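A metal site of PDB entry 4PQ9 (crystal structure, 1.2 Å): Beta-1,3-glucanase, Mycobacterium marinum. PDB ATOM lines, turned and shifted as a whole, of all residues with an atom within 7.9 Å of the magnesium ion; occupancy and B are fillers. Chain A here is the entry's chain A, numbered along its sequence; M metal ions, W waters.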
ATOM      1  N   ASP A  33      -7.808  -8.763  22.844  1.00  0.00           N
ATOM      2  CA  ASP A  33      -7.762  -9.375  21.523  1.00  0.00           C
ATOM      3  C   ASP A  33      -9.193  -9.519  21.063  1.00  0.00           C
ATOM      4  O   ASP A  33     -10.032 -10.086  21.756  1.00  0.00           O
ATOM      5  CB  ASP A  33      -7.042 -10.736  21.534  1.00  0.00           C
ATOM      6  CG  ASP A  33      -6.605 -11.173  20.140  1.00  0.00           C
ATOM      7  OD1 ASP A  33      -7.061 -10.567  19.137  1.00  0.00           O
ATOM      8  OD2 ASP A  33      -5.818 -12.143  20.098  1.00  0.00           O
ATOM      9  N   GLU A  34      -9.445  -8.993  19.871  1.00  0.00           N
ATOM     10  CA  GLU A  34     -10.741  -9.090  19.216  1.00  0.00           C
ATOM     11  C   GLU A  34     -10.842 -10.306  18.292  1.00  0.00           C
ATOM     12  O   GLU A  34     -11.914 -10.600  17.753  1.00  0.00           O
ATOM     13  CB  GLU A  34     -11.002  -7.789  18.440  1.00  0.00           C
ATOM     14  CG  GLU A  34     -10.958  -6.553  19.308  1.00  0.00           C
ATOM     15  CD  GLU A  34     -11.921  -6.587  20.476  1.00  0.00           C
ATOM     16  OE1 GLU A  34     -13.060  -7.071  20.301  1.00  0.00           O
ATOM     17  OE2 GLU A  34     -11.583  -6.056  21.567  1.00  0.00           O
ATOM     18  N   PHE A  35      -9.721 -11.019  18.100  1.00  0.00           N
ATOM     19  CA  PHE A  35      -9.717 -12.251  17.304  1.00  0.00           C
ATOM     20  C   PHE A  35     -10.202 -12.034  15.882  1.00  0.00           C
ATOM     21  O   PHE A  35     -10.848 -12.874  15.292  1.00  0.00           O
ATOM     22  CB  PHE A  35     -10.460 -13.410  18.021  1.00  0.00           C
ATOM     23  CG  PHE A  35      -9.852 -13.779  19.343  1.00  0.00           C
ATOM     24  CD1 PHE A  35      -8.575 -14.313  19.417  1.00  0.00           C
ATOM     25  CD2 PHE A  35     -10.545 -13.607  20.520  1.00  0.00           C
ATOM     26  CE1 PHE A  35      -8.032 -14.689  20.616  1.00  0.00           C
ATOM     27  CE2 PHE A  35     -10.004 -13.974  21.729  1.00  0.00           C
ATOM     28  CZ  PHE A  35      -8.729 -14.500  21.776  1.00  0.00           C
ATOM     29  N   ASP A  36      -9.837 -10.875  15.335  1.00  0.00           N
ATOM     30  CA  ASP A  36     -10.164 -10.547  13.977  1.00  0.00           C
ATOM     31  C   ASP A  36      -9.100 -11.074  13.032  1.00  0.00           C
ATOM     32  O   ASP A  36      -7.916 -11.178  13.368  1.00  0.00           O
ATOM     33  CB  ASP A  36     -10.320  -9.035  13.824  1.00  0.00           C
ATOM     34  CG  ASP A  36     -11.579  -8.532  14.467  1.00  0.00           C
ATOM     35  OD1 ASP A  36     -12.629  -9.190  14.305  1.00  0.00           O
ATOM     36  OD2 ASP A  36     -11.527  -7.468  15.126  1.00  0.00           O
ATOM     37  N   GLY A  37      -9.559 -11.394  11.837  1.00  0.00           N
ATOM     38  CA  GLY A  37      -8.686 -11.880  10.783  1.00  0.00           C
ATOM     39  C   GLY A  37      -9.375 -12.962  10.006  1.00  0.00           C
ATOM     40  O   GLY A  37     -10.442 -13.430  10.381  1.00  0.00           O
ATOM     41  N   ASP A  82     -12.074 -17.916  13.008  1.00  0.00           N
ATOM     42  CA  ASP A  82     -13.108 -18.306  12.074  1.00  0.00           C
ATOM     43  C   ASP A  82     -13.416 -17.306  10.977  1.00  0.00           C
ATOM     44  O   ASP A  82     -14.249 -17.597  10.116  1.00  0.00           O
ATOM     45  CB  ASP A  82     -14.402 -18.708  12.797  1.00  0.00           C
ATOM     46  CG  ASP A  82     -15.102 -17.564  13.505  1.00  0.00           C
ATOM     47  OD1 ASP A  82     -14.606 -16.426  13.494  1.00  0.00           O
ATOM     48  OD2 ASP A  82     -16.181 -17.837  14.095  1.00  0.00           O
ATOM     49  N   LYS A  84     -14.929 -14.548  11.484  1.00  0.00           N
ATOM     50  CA  LYS A  84     -16.101 -13.853  11.953  1.00  0.00           C
ATOM     51  C   LYS A  84     -15.851 -13.189  13.299  1.00  0.00           C
ATOM     52  O   LYS A  84     -16.787 -12.881  14.030  1.00  0.00           O
ATOM     53  CB  LYS A  84     -17.283 -14.837  12.049  1.00  0.00           C
ATOM     54  CG  LYS A  84     -17.572 -15.545  10.731  1.00  0.00           C
ATOM     55  CD  LYS A  84     -18.711 -16.540  10.873  1.00  0.00           C
ATOM     56  CE  LYS A  84     -19.356 -16.883   9.545  1.00  0.00           C
ATOM     57  NZ  LYS A  84     -18.416 -17.347   8.500  1.00  0.00           N
ATOM     58  N   SER A  85     -14.575 -12.913  13.577  1.00  0.00           N
ATOM     59  CA  SER A  85     -14.134 -12.248  14.800  1.00  0.00           C
ATOM     60  C   SER A  85     -13.999 -13.175  16.009  1.00  0.00           C
ATOM     61  O   SER A  85     -13.867 -12.699  17.142  1.00  0.00           O
ATOM     62  CB  SER A  85     -15.025 -11.046  15.147  1.00  0.00           C
ATOM     63  OG  SER A  85     -14.332 -10.177  16.042  1.00  0.00           O
ATOM     64  N   ASN A  86     -13.983 -14.488  15.770  1.00  0.00           N
ATOM     65  CA  ASN A  86     -13.860 -15.431  16.872  1.00  0.00           C
ATOM     66  C   ASN A  86     -12.638 -16.318  16.765  1.00  0.00           C
ATOM     67  O   ASN A  86     -12.291 -16.841  15.728  1.00  0.00           O
ATOM     68  CB  ASN A  86     -15.067 -16.348  16.929  1.00  0.00           C
ATOM     69  CG  ASN A  86     -16.367 -15.607  16.898  1.00  0.00           C
ATOM     70  OD1 ASN A  86     -16.586 -14.689  17.689  1.00  0.00           O
ATOM     71  ND2 ASN A  86     -17.245 -16.010  15.979  1.00  0.00           N
ATOM     72  N   LEU A  87     -12.003 -16.516  17.934  1.00  0.00           N
ATOM     73  CA  LEU A  87     -11.181 -17.689  18.194  1.00  0.00           C
ATOM     74  C   LEU A  87     -12.097 -18.905  18.218  1.00  0.00           C
ATOM     75  O   LEU A  87     -13.185 -18.889  18.813  1.00  0.00           O
ATOM     76  CB  LEU A  87     -10.526 -17.542  19.557  1.00  0.00           C
ATOM     77  CG  LEU A  87      -9.747 -18.751  20.053  1.00  0.00           C
ATOM     78  CD1 LEU A  87      -8.409 -18.803  19.321  1.00  0.00           C
ATOM     79  CD2 LEU A  87      -9.547 -18.661  21.561  1.00  0.00           C
ATOM     80  N   ARG A 118     -16.083 -12.744  25.757  1.00  0.00           N
ATOM     81  CA  ARG A 118     -17.351 -13.066  25.128  1.00  0.00           C
ATOM     82  C   ARG A 118     -17.209 -14.439  24.490  1.00  0.00           C
ATOM     83  O   ARG A 118     -16.353 -14.605  23.620  1.00  0.00           O
ATOM     84  CB  ARG A 118     -17.723 -12.002  24.090  1.00  0.00           C
ATOM     85  CG  ARG A 118     -19.060 -12.267  23.414  1.00  0.00           C
ATOM     86  CD  ARG A 118     -19.569 -11.057  22.630  1.00  0.00           C
ATOM     87  NE  ARG A 118     -20.916 -11.320  22.110  1.00  0.00           N
ATOM     88  CZ  ARG A 118     -21.194 -11.875  20.942  1.00  0.00           C
ATOM     89  NH1 ARG A 118     -20.244 -12.105  20.048  1.00  0.00           N
ATOM     90  NH2 ARG A 118     -22.444 -12.169  20.635  1.00  0.00           N
ATOM     91  N   TRP A 179     -24.378 -17.141  23.253  1.00  0.00           N
ATOM     92  CA  TRP A 179     -23.320 -16.147  23.476  1.00  0.00           C
ATOM     93  C   TRP A 179     -23.514 -15.462  24.804  1.00  0.00           C
ATOM     94  O   TRP A 179     -24.609 -15.022  25.126  1.00  0.00           O
ATOM     95  CB  TRP A 179     -23.333 -15.098  22.366  1.00  0.00           C
ATOM     96  CG  TRP A 179     -22.673 -15.491  21.131  1.00  0.00           C
ATOM     97  CD1 TRP A 179     -23.265 -15.786  19.922  1.00  0.00           C
ATOM     98  CD2 TRP A 179     -21.268 -15.574  20.915  1.00  0.00           C
ATOM     99  NE1 TRP A 179     -22.296 -16.065  18.999  1.00  0.00           N
ATOM    100  CE2 TRP A 179     -21.063 -15.954  19.580  1.00  0.00           C
ATOM    101  CE3 TRP A 179     -20.160 -15.387  21.731  1.00  0.00           C
ATOM    102  CZ2 TRP A 179     -19.787 -16.137  19.045  1.00  0.00           C
ATOM    103  CZ3 TRP A 179     -18.889 -15.578  21.193  1.00  0.00           C
ATOM    104  CH2 TRP A 179     -18.722 -15.941  19.866  1.00  0.00           C
ATOM    105  N   VAL A 251     -14.689 -17.718  20.923  1.00  0.00           N
ATOM    106  CA  VAL A 251     -14.416 -16.558  21.770  1.00  0.00           C
ATOM    107  C   VAL A 251     -14.282 -15.318  20.893  1.00  0.00           C
ATOM    108  O   VAL A 251     -13.391 -15.238  20.064  1.00  0.00           O
ATOM    109  CB  VAL A 251     -13.143 -16.752  22.633  1.00  0.00           C
ATOM    110  CG1 VAL A 251     -13.008 -15.595  23.591  1.00  0.00           C
ATOM    111  CG2 VAL A 251     -13.154 -18.074  23.399  1.00  0.00           C
ATOM    112  N   ASP A 252     -15.196 -14.379  21.044  1.00  0.00           N
ATOM    113  CA  ASP A 252     -15.182 -13.184  20.222  1.00  0.00           C
ATOM    114  C   ASP A 252     -14.113 -12.193  20.678  1.00  0.00           C
ATOM    115  O   ASP A 252     -13.526 -11.468  19.853  1.00  0.00           O
ATOM    116  CB  ASP A 252     -16.579 -12.546  20.258  1.00  0.00           C
ATOM    117  CG  ASP A 252     -16.790 -11.388  19.300  1.00  0.00           C
ATOM    118  OD1 ASP A 252     -15.954 -11.094  18.416  1.00  0.00           O
ATOM    119  OD2 ASP A 252     -17.885 -10.763  19.422  1.00  0.00           O
ATOM    120  N   TRP A 253     -13.833 -12.152  21.978  1.00  0.00           N
ATOM    121  CA  TRP A 253     -12.857 -11.201  22.459  1.00  0.00           C
ATOM    122  C   TRP A 253     -12.512 -11.524  23.905  1.00  0.00           C
ATOM    123  O   TRP A 253     -13.296 -12.171  24.624  1.00  0.00           O
ATOM    124  CB  TRP A 253     -13.326  -9.744  22.333  1.00  0.00           C
ATOM    125  CG  TRP A 253     -14.707  -9.413  22.658  1.00  0.00           C
ATOM    126  CD1 TRP A 253     -15.734  -9.153  21.767  1.00  0.00           C
ATOM    127  CD2 TRP A 253     -15.236  -9.133  23.943  1.00  0.00           C
ATOM    128  NE1 TRP A 253     -16.849  -8.765  22.443  1.00  0.00           N
ATOM    129  CE2 TRP A 253     -16.586  -8.724  23.781  1.00  0.00           C
ATOM    130  CE3 TRP A 253     -14.716  -9.189  25.244  1.00  0.00           C
ATOM    131  CZ2 TRP A 253     -17.414  -8.363  24.835  1.00  0.00           C
ATOM    132  CZ3 TRP A 253     -15.551  -8.824  26.292  1.00  0.00           C
ATOM    133  CH2 TRP A 253     -16.880  -8.442  26.100  1.00  0.00           C
ATOM    134  N   VAL A 254     -11.327 -11.044  24.289  1.00  0.00           N
ATOM    135  CA  VAL A 254     -10.856 -10.915  25.680  1.00  0.00           C
ATOM    136  C   VAL A 254     -10.463  -9.463  25.865  1.00  0.00           C
ATOM    137  O   VAL A 254      -9.739  -8.921  25.040  1.00  0.00           O
ATOM    138  CB  VAL A 254      -9.639 -11.829  25.986  1.00  0.00           C
ATOM    139  CG1 VAL A 254      -8.985 -11.504  27.323  1.00  0.00           C
ATOM    140  CG2 VAL A 254     -10.040 -13.294  25.872  1.00  0.00           C
ATOM    141  N   ARG A 255     -10.929  -8.855  26.940  1.00  0.00           N
ATOM    142  CA  ARG A 255     -10.669  -7.438  27.219  1.00  0.00           C
ATOM    143  C   ARG A 255     -10.348  -7.276  28.695  1.00  0.00           C
ATOM    144  O   ARG A 255     -11.010  -7.870  29.560  1.00  0.00           O
ATOM    145  CB  ARG A 255     -11.852  -6.559  26.843  1.00  0.00           C
ATOM    146  CG  ARG A 255     -12.136  -6.496  25.352  1.00  0.00           C
ATOM    147  CD  ARG A 255     -13.489  -5.915  25.053  1.00  0.00           C
ATOM    148  NE  ARG A 255     -13.744  -5.914  23.616  1.00  0.00           N
ATOM    149  CZ  ARG A 255     -14.930  -5.648  23.083  1.00  0.00           C
ATOM    150  NH1 ARG A 255     -15.940  -5.312  23.855  1.00  0.00           N
ATOM    151  NH2 ARG A 255     -15.094  -5.714  21.784  1.00  0.00           N
HETATM  152 MG    MG M   1     -13.958 -10.817  17.987  1.00  0.00          MG
HETATM  153  O   HOH W   1     -14.212  -8.833  18.600  1.00  0.00           O
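The magnesium ion is bound by O of Asp 252, 2.0 Å away.
The magnesium ion is bound by OD1 of Asp 252 (2.1 Å).
The magnesium ion is bound by the backbone carbonyl oxygen (O) of Ser 85 (2.1 Å).
The magnesium ion is bound by O of Glu 34 (2.1 Å).
The magnesium ion is bound by OG of Ser 85, at 2.1 Å.
The magnesium ion is bound by water W1, at 2.1 Å.
The magnesium ion has six donor atoms within binding distance.
OE1 of Glu 34 lies within salt-bridge range of NH2 of Arg 255 (2.9 Å).
OG of Ser 85 lies close to OD1 of Asp 36.
OD2 of Asp 252 lies within salt-bridge range of NH1 of Arg 118 (2.8 Å).
Of the 17 residues printed, 3 come within 4 Å of the magnesium ion.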
